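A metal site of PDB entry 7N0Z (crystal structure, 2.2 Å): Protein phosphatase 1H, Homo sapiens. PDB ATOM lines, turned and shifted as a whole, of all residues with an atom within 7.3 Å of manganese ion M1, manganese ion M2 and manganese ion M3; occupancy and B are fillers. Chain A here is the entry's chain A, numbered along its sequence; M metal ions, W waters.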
ATOM      1  N   LYS A  60      -2.287  -4.920  11.029  1.00  0.00           N
ATOM      2  CA  LYS A  60      -2.157  -3.800  10.102  1.00  0.00           C
ATOM      3  C   LYS A  60      -1.651  -4.236   8.732  1.00  0.00           C
ATOM      4  O   LYS A  60      -2.041  -3.640   7.717  1.00  0.00           O
ATOM      5  CB  LYS A  60      -1.260  -2.722  10.693  1.00  0.00           C
ATOM      6  CG  LYS A  60       0.009  -3.227  11.359  1.00  0.00           C
ATOM      7  CD  LYS A  60       0.864  -2.047  11.778  1.00  0.00           C
ATOM      8  CE  LYS A  60       2.323  -2.432  11.954  1.00  0.00           C
ATOM      9  NZ  LYS A  60       3.053  -1.405  12.745  1.00  0.00           N
ATOM     10  N   SER A  61      -0.804  -5.267   8.663  1.00  0.00           N
ATOM     11  CA  SER A  61      -0.386  -5.857   7.409  1.00  0.00           C
ATOM     12  C   SER A  61      -0.582  -7.358   7.479  1.00  0.00           C
ATOM     13  O   SER A  61      -0.340  -7.976   8.526  1.00  0.00           O
ATOM     14  CB  SER A  61       1.073  -5.523   7.067  1.00  0.00           C
ATOM     15  OG  SER A  61       1.943  -5.880   8.115  1.00  0.00           O
ATOM     16  N   ASN A  64       3.904 -10.658   8.285  1.00  0.00           N
ATOM     17  CA  ASN A  64       4.930 -10.140   9.180  1.00  0.00           C
ATOM     18  C   ASN A  64       6.073  -9.585   8.343  1.00  0.00           C
ATOM     19  O   ASN A  64       6.719 -10.326   7.590  1.00  0.00           O
ATOM     20  CB  ASN A  64       5.416 -11.241  10.120  1.00  0.00           C
ATOM     21  CG  ASN A  64       6.364 -10.732  11.202  1.00  0.00           C
ATOM     22  OD1 ASN A  64       7.075  -9.742  11.010  1.00  0.00           O
ATOM     23  ND2 ASN A  64       6.373 -11.417  12.332  1.00  0.00           N
ATOM     24  N   GLU A  65       6.318  -8.287   8.449  1.00  0.00           N
ATOM     25  CA  GLU A  65       7.293  -7.622   7.603  1.00  0.00           C
ATOM     26  C   GLU A  65       8.666  -7.476   8.249  1.00  0.00           C
ATOM     27  O   GLU A  65       9.584  -6.952   7.609  1.00  0.00           O
ATOM     28  CB  GLU A  65       6.760  -6.260   7.167  1.00  0.00           C
ATOM     29  CG  GLU A  65       5.555  -6.373   6.230  1.00  0.00           C
ATOM     30  CD  GLU A  65       5.095  -5.030   5.687  1.00  0.00           C
ATOM     31  OE1 GLU A  65       5.210  -4.015   6.397  1.00  0.00           O
ATOM     32  OE2 GLU A  65       4.621  -4.994   4.529  1.00  0.00           O
ATOM     33  N   ASP A  66       8.823  -7.942   9.485  1.00  0.00           N
ATOM     34  CA  ASP A  66      10.162  -8.114  10.040  1.00  0.00           C
ATOM     35  C   ASP A  66      10.822  -9.335   9.412  1.00  0.00           C
ATOM     36  O   ASP A  66      10.181 -10.348   9.162  1.00  0.00           O
ATOM     37  CB  ASP A  66      10.112  -8.281  11.562  1.00  0.00           C
ATOM     38  CG  ASP A  66       9.801  -6.995  12.287  1.00  0.00           C
ATOM     39  OD1 ASP A  66       9.848  -6.992  13.528  1.00  0.00           O
ATOM     40  OD2 ASP A  66       9.491  -5.989  11.616  1.00  0.00           O
ATOM     41  N   PHE A 122      15.685  -6.837  10.107  1.00  0.00           N
ATOM     42  CA  PHE A 122      15.177  -5.916   9.098  1.00  0.00           C
ATOM     43  C   PHE A 122      13.695  -5.683   9.351  1.00  0.00           C
ATOM     44  O   PHE A 122      12.925  -6.640   9.427  1.00  0.00           O
ATOM     45  CB  PHE A 122      15.408  -6.458   7.690  1.00  0.00           C
ATOM     46  CG  PHE A 122      16.820  -6.916   7.433  1.00  0.00           C
ATOM     47  CD1 PHE A 122      17.781  -6.024   6.959  1.00  0.00           C
ATOM     48  CD2 PHE A 122      17.189  -8.220   7.683  1.00  0.00           C
ATOM     49  CE1 PHE A 122      19.078  -6.451   6.726  1.00  0.00           C
ATOM     50  CE2 PHE A 122      18.487  -8.644   7.464  1.00  0.00           C
ATOM     51  CZ  PHE A 122      19.431  -7.761   6.979  1.00  0.00           C
ATOM     52  N   ASP A 123      13.318  -4.420   9.492  1.00  0.00           N
ATOM     53  CA  ASP A 123      11.927  -4.033   9.702  1.00  0.00           C
ATOM     54  C   ASP A 123      11.411  -3.455   8.388  1.00  0.00           C
ATOM     55  O   ASP A 123      11.690  -2.294   8.054  1.00  0.00           O
ATOM     56  CB  ASP A 123      11.805  -3.035  10.848  1.00  0.00           C
ATOM     57  CG  ASP A 123      10.364  -2.699  11.189  1.00  0.00           C
ATOM     58  OD1 ASP A 123       9.450  -3.101  10.444  1.00  0.00           O
ATOM     59  OD2 ASP A 123      10.151  -2.023  12.218  1.00  0.00           O
ATOM     60  N   GLY A 124      10.675  -4.273   7.644  1.00  0.00           N
ATOM     61  CA  GLY A 124      10.162  -3.832   6.373  1.00  0.00           C
ATOM     62  C   GLY A 124       8.935  -2.954   6.515  1.00  0.00           C
ATOM     63  O   GLY A 124       8.214  -2.995   7.512  1.00  0.00           O
ATOM     64  N   HIS A 125       8.704  -2.124   5.500  1.00  0.00           N
ATOM     65  CA  HIS A 125       7.532  -1.282   5.424  1.00  0.00           C
ATOM     66  C   HIS A 125       7.096  -1.155   3.970  1.00  0.00           C
ATOM     67  O   HIS A 125       7.914  -1.245   3.048  1.00  0.00           O
ATOM     68  CB  HIS A 125       7.785   0.114   6.016  1.00  0.00           C
ATOM     69  CG  HIS A 125       8.995   0.802   5.471  1.00  0.00           C
ATOM     70  ND1 HIS A 125      10.142   0.987   6.216  1.00  0.00           N
ATOM     71  CD2 HIS A 125       9.232   1.369   4.263  1.00  0.00           C
ATOM     72  CE1 HIS A 125      11.040   1.629   5.480  1.00  0.00           C
ATOM     73  NE2 HIS A 125      10.520   1.870   4.291  1.00  0.00           N
ATOM     74  N   ALA A 126       5.787  -0.970   3.777  1.00  0.00           N
ATOM     75  CA  ALA A 126       5.184  -0.854   2.448  1.00  0.00           C
ATOM     76  C   ALA A 126       5.504  -2.079   1.589  1.00  0.00           C
ATOM     77  O   ALA A 126       5.781  -1.954   0.393  1.00  0.00           O
ATOM     78  CB  ALA A 126       5.612   0.428   1.748  1.00  0.00           C
ATOM     79  N   GLY A 127       5.474  -3.259   2.199  1.00  0.00           N
ATOM     80  CA  GLY A 127       5.796  -4.485   1.494  1.00  0.00           C
ATOM     81  C   GLY A 127       6.884  -5.292   2.179  1.00  0.00           C
ATOM     82  O   GLY A 127       7.640  -4.747   2.994  1.00  0.00           O
ATOM     83  N   GLY A 205      10.566  -0.927   1.483  1.00  0.00           N
ATOM     84  CA  GLY A 205      11.904  -0.735   1.994  1.00  0.00           C
ATOM     85  C   GLY A 205      12.006  -1.370   3.364  1.00  0.00           C
ATOM     86  O   GLY A 205      11.065  -2.002   3.849  1.00  0.00           O
ATOM     87  N   THR A 207      14.384  -1.039   7.368  1.00  0.00           N
ATOM     88  CA  THR A 207      15.524  -0.695   8.196  1.00  0.00           C
ATOM     89  C   THR A 207      16.482  -1.882   8.245  1.00  0.00           C
ATOM     90  O   THR A 207      16.139  -3.011   7.892  1.00  0.00           O
ATOM     91  CB  THR A 207      15.078  -0.306   9.606  1.00  0.00           C
ATOM     92  OG1 THR A 207      14.479  -1.438  10.242  1.00  0.00           O
ATOM     93  CG2 THR A 207      14.056   0.816   9.547  1.00  0.00           C
ATOM     94  N   ASP A 225      15.496   2.496  12.699  1.00  0.00           N
ATOM     95  CA  ASP A 225      15.054   2.821  14.045  1.00  0.00           C
ATOM     96  C   ASP A 225      14.831   1.600  14.920  1.00  0.00           C
ATOM     97  O   ASP A 225      14.156   1.696  15.953  1.00  0.00           O
ATOM     98  CB  ASP A 225      13.788   3.691  14.000  1.00  0.00           C
ATOM     99  CG  ASP A 225      12.561   2.926  13.520  1.00  0.00           C
ATOM    100  OD1 ASP A 225      12.705   1.853  12.905  1.00  0.00           O
ATOM    101  OD2 ASP A 225      11.437   3.421  13.752  1.00  0.00           O
ATOM    102  N   SER A 226      15.375   0.439  14.543  1.00  0.00           N
ATOM    103  CA  SER A 226      15.543  -0.632  15.513  1.00  0.00           C
ATOM    104  C   SER A 226      16.631  -0.242  16.505  1.00  0.00           C
ATOM    105  O   SER A 226      17.305   0.777  16.358  1.00  0.00           O
ATOM    106  CB  SER A 226      15.880  -1.947  14.810  1.00  0.00           C
ATOM    107  OG  SER A 226      14.845  -2.328  13.916  1.00  0.00           O
ATOM    108  N   THR A 244      15.692   9.263  12.463  1.00  0.00           N
ATOM    109  CA  THR A 244      14.331   9.739  12.254  1.00  0.00           C
ATOM    110  C   THR A 244      14.381  11.181  11.750  1.00  0.00           C
ATOM    111  O   THR A 244      15.456  11.790  11.750  1.00  0.00           O
ATOM    112  CB  THR A 244      13.539   9.635  13.569  1.00  0.00           C
ATOM    113  OG1 THR A 244      13.865  10.731  14.421  1.00  0.00           O
ATOM    114  CG2 THR A 244      13.820   8.314  14.295  1.00  0.00           C
ATOM    115  N   LYS A 315       7.730  10.109  17.863  1.00  0.00           N
ATOM    116  CA  LYS A 315       7.360   9.042  16.947  1.00  0.00           C
ATOM    117  C   LYS A 315       6.427   9.513  15.842  1.00  0.00           C
ATOM    118  O   LYS A 315       6.169   8.732  14.906  1.00  0.00           O
ATOM    119  CB  LYS A 315       6.701   7.896  17.705  1.00  0.00           C
ATOM    120  CG  LYS A 315       7.577   7.226  18.740  1.00  0.00           C
ATOM    121  CD  LYS A 315       6.742   6.250  19.561  1.00  0.00           C
ATOM    122  CE  LYS A 315       7.455   5.844  20.839  1.00  0.00           C
ATOM    123  NZ  LYS A 315       6.499   5.446  21.900  1.00  0.00           N
ATOM    124  N   GLY A 324       8.613   8.359   8.775  1.00  0.00           N
ATOM    125  CA  GLY A 324       9.147   8.660  10.092  1.00  0.00           C
ATOM    126  C   GLY A 324      10.488   8.039  10.391  1.00  0.00           C
ATOM    127  O   GLY A 324      10.985   8.162  11.514  1.00  0.00           O
ATOM    128  N   VAL A 325      11.100   7.364   9.417  1.00  0.00           N
ATOM    129  CA  VAL A 325      12.437   6.798   9.562  1.00  0.00           C
ATOM    130  C   VAL A 325      13.227   7.160   8.318  1.00  0.00           C
ATOM    131  O   VAL A 325      12.713   7.063   7.189  1.00  0.00           O
ATOM    132  CB  VAL A 325      12.391   5.263   9.776  1.00  0.00           C
ATOM    133  CG1 VAL A 325      11.636   4.577   8.647  1.00  0.00           C
ATOM    134  CG2 VAL A 325      13.802   4.700   9.919  1.00  0.00           C
ATOM    135  N   THR A 373      13.424  -4.987  16.921  1.00  0.00           N
ATOM    136  CA  THR A 373      12.758  -3.998  16.089  1.00  0.00           C
ATOM    137  C   THR A 373      11.930  -3.063  16.972  1.00  0.00           C
ATOM    138  O   THR A 373      11.698  -3.326  18.159  1.00  0.00           O
ATOM    139  CB  THR A 373      11.875  -4.678  15.049  1.00  0.00           C
ATOM    140  OG1 THR A 373      10.957  -5.558  15.702  1.00  0.00           O
ATOM    141  CG2 THR A 373      12.740  -5.478  14.078  1.00  0.00           C
ATOM    142  N   ASP A 374      11.460  -1.956  16.374  1.00  0.00           N
ATOM    143  CA  ASP A 374      10.729  -0.982  17.164  1.00  0.00           C
ATOM    144  C   ASP A 374       9.403  -1.514  17.708  1.00  0.00           C
ATOM    145  O   ASP A 374       8.777  -0.840  18.522  1.00  0.00           O
ATOM    146  CB  ASP A 374      10.495   0.299  16.345  1.00  0.00           C
ATOM    147  CG  ASP A 374       9.747   0.042  15.052  1.00  0.00           C
ATOM    148  OD1 ASP A 374       9.205  -1.065  14.861  1.00  0.00           O
ATOM    149  OD2 ASP A 374       9.703   0.960  14.206  1.00  0.00           O
ATOM    150  N   GLY A 375       8.978  -2.712  17.288  1.00  0.00           N
ATOM    151  CA  GLY A 375       7.808  -3.321  17.898  1.00  0.00           C
ATOM    152  C   GLY A 375       7.997  -3.609  19.372  1.00  0.00           C
ATOM    153  O   GLY A 375       7.024  -3.726  20.119  1.00  0.00           O
ATOM    154  N   LEU A 376       9.249  -3.737  19.815  1.00  0.00           N
ATOM    155  CA  LEU A 376       9.544  -3.848  21.240  1.00  0.00           C
ATOM    156  C   LEU A 376       9.762  -2.482  21.863  1.00  0.00           C
ATOM    157  O   LEU A 376       9.148  -2.159  22.886  1.00  0.00           O
ATOM    158  CB  LEU A 376      10.780  -4.728  21.456  1.00  0.00           C
ATOM    159  CG  LEU A 376      11.140  -4.994  22.920  1.00  0.00           C
ATOM    160  CD1 LEU A 376      10.388  -6.201  23.455  1.00  0.00           C
ATOM    161  CD2 LEU A 376      12.641  -5.152  23.136  1.00  0.00           C
ATOM    162  N   ASP A 378       8.935   0.490  21.079  1.00  0.00           N
ATOM    163  CA  ASP A 378       7.879   1.495  21.081  1.00  0.00           C
ATOM    164  C   ASP A 378       7.004   1.450  22.317  1.00  0.00           C
ATOM    165  O   ASP A 378       6.232   2.388  22.540  1.00  0.00           O
ATOM    166  CB  ASP A 378       7.010   1.356  19.826  1.00  0.00           C
ATOM    167  CG  ASP A 378       7.666   1.959  18.589  1.00  0.00           C
ATOM    168  OD1 ASP A 378       8.643   2.728  18.739  1.00  0.00           O
ATOM    169  OD2 ASP A 378       7.200   1.658  17.467  1.00  0.00           O
ATOM    170  N   ASP A 435       2.497  -4.065  16.654  1.00  0.00           N
ATOM    171  CA  ASP A 435       3.444  -4.196  15.557  1.00  0.00           C
ATOM    172  C   ASP A 435       4.006  -5.622  15.490  1.00  0.00           C
ATOM    173  O   ASP A 435       3.819  -6.441  16.390  1.00  0.00           O
ATOM    174  CB  ASP A 435       4.573  -3.181  15.733  1.00  0.00           C
ATOM    175  CG  ASP A 435       5.398  -2.992  14.482  1.00  0.00           C
ATOM    176  OD1 ASP A 435       5.029  -3.540  13.430  1.00  0.00           O
ATOM    177  OD2 ASP A 435       6.414  -2.271  14.556  1.00  0.00           O
ATOM    178  N   ASP A 436       4.701  -5.908  14.389  1.00  0.00           N
ATOM    179  CA  ASP A 436       5.619  -7.038  14.388  1.00  0.00           C
ATOM    180  C   ASP A 436       6.713  -6.799  15.419  1.00  0.00           C
ATOM    181  O   ASP A 436       7.199  -5.674  15.571  1.00  0.00           O
ATOM    182  CB  ASP A 436       6.240  -7.255  13.015  1.00  0.00           C
ATOM    183  CG  ASP A 436       5.215  -7.328  11.901  1.00  0.00           C
ATOM    184  OD1 ASP A 436       4.245  -8.100  12.037  1.00  0.00           O
ATOM    185  OD2 ASP A 436       5.389  -6.631  10.880  1.00  0.00           O
ATOM    186  N   ILE A 437       7.071  -7.846  16.151  1.00  0.00           N
ATOM    187  CA  ILE A 437       8.096  -7.754  17.179  1.00  0.00           C
ATOM    188  C   ILE A 437       9.100  -8.888  16.964  1.00  0.00           C
ATOM    189  O   ILE A 437       8.703 -10.050  16.856  1.00  0.00           O
ATOM    190  CB  ILE A 437       7.504  -7.839  18.601  1.00  0.00           C
ATOM    191  CG1 ILE A 437       6.300  -6.906  18.743  1.00  0.00           C
ATOM    192  CG2 ILE A 437       8.558  -7.512  19.633  1.00  0.00           C
ATOM    193  CD1 ILE A 437       5.574  -7.036  20.063  1.00  0.00           C
HETATM  194 MN    MN M   1       8.186  -2.058  13.286  1.00  0.00          MN
HETATM  195 MN    MN M   2       7.544  -2.877   9.658  1.00  0.00          MN
HETATM  196 MN    MN M   3       9.400   3.160  14.129  1.00  0.00          MN
HETATM  197  O   HOH W   1       7.003   4.127  14.625  1.00  0.00           O
HETATM  198  O   HOH W   2       8.383   5.518  13.475  1.00  0.00           O
HETATM  199  O   HOH W   3       7.828  -0.032  12.276  1.00  0.00           O
HETATM  200  O   HOH W   4       6.703  -2.344  11.664  1.00  0.00           O
HETATM  201  O   HOH W   5       7.770  -0.668   9.848  1.00  0.00           O
HETATM  202  O   HOH W   6       7.733  -5.168  10.414  1.00  0.00           O
HETATM  203  O   HOH W   7       8.607  -4.264  13.778  1.00  0.00           O
HETATM  204  O   HOH W   8       9.957   3.565  16.024  1.00  0.00           O
HETATM  205  O   HOH W   9       5.328  -3.214   8.809  1.00  0.00           O
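The side-chain carboxylate (OD1) of Asp 435 lies within salt-bridge range of the side-chain amino group (NZ) of Lys 60, 3.0 Å away. O of Asp 123 is in hydrogen-bond range of N of Thr 207. The backbone NH of Gly 124 lies within hydrogen-bond range of the backbone carbonyl oxygen of Glu 65 (2.9 Å).
Manganese ion M1 is bound by the side-chain carboxylate of Asp 374, the side-chain carboxylate of Asp 435, water W4, the side-chain carboxylate of Asp 123, water W3 and water W7.
Of the 27 residues printed, 3 come within 4 Å of manganese ion M1. The nearest printed residue that does not touch manganese ion M1 is Gly 375 (4.1 Å).
Two residues have an atom within 4 Å of manganese ion M2: Asp 123 and Gly 124.
Manganese ion M2 is bound by the side-chain carboxylate (OD1) of Asp 123 (2.1 Å), water W5 (2.2 Å), water W4 (2.2 Å), the backbone carbonyl oxygen (O) of Gly 124 (2.3 Å), water W9 (2.4 Å) and water W6 (2.4 Å). Manganese ion M2 has six donor atoms within binding distance.
Water W8 binds manganese ion M3. OD2 of Asp 225 binds manganese ion M3 (2.1 Å). OD2 of Asp 374 binds manganese ion M3 (2.2 Å). Manganese ion M3 is bound by water W1 (2.6 Å). Manganese ion M3 is bound by water W2, at 2.6 Å.
Water W7 lies within hydrogen-bond range of O of Asp 436 (2.7 Å), OD2 of Asp 66 (2.9 Å) and OG1 of Thr 373 (3.3 Å). Water W6 bridges the side-chain carboxylate of Asp 436 (2.8 Å) and the backbone NH of Asp 66 (3.1 Å).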
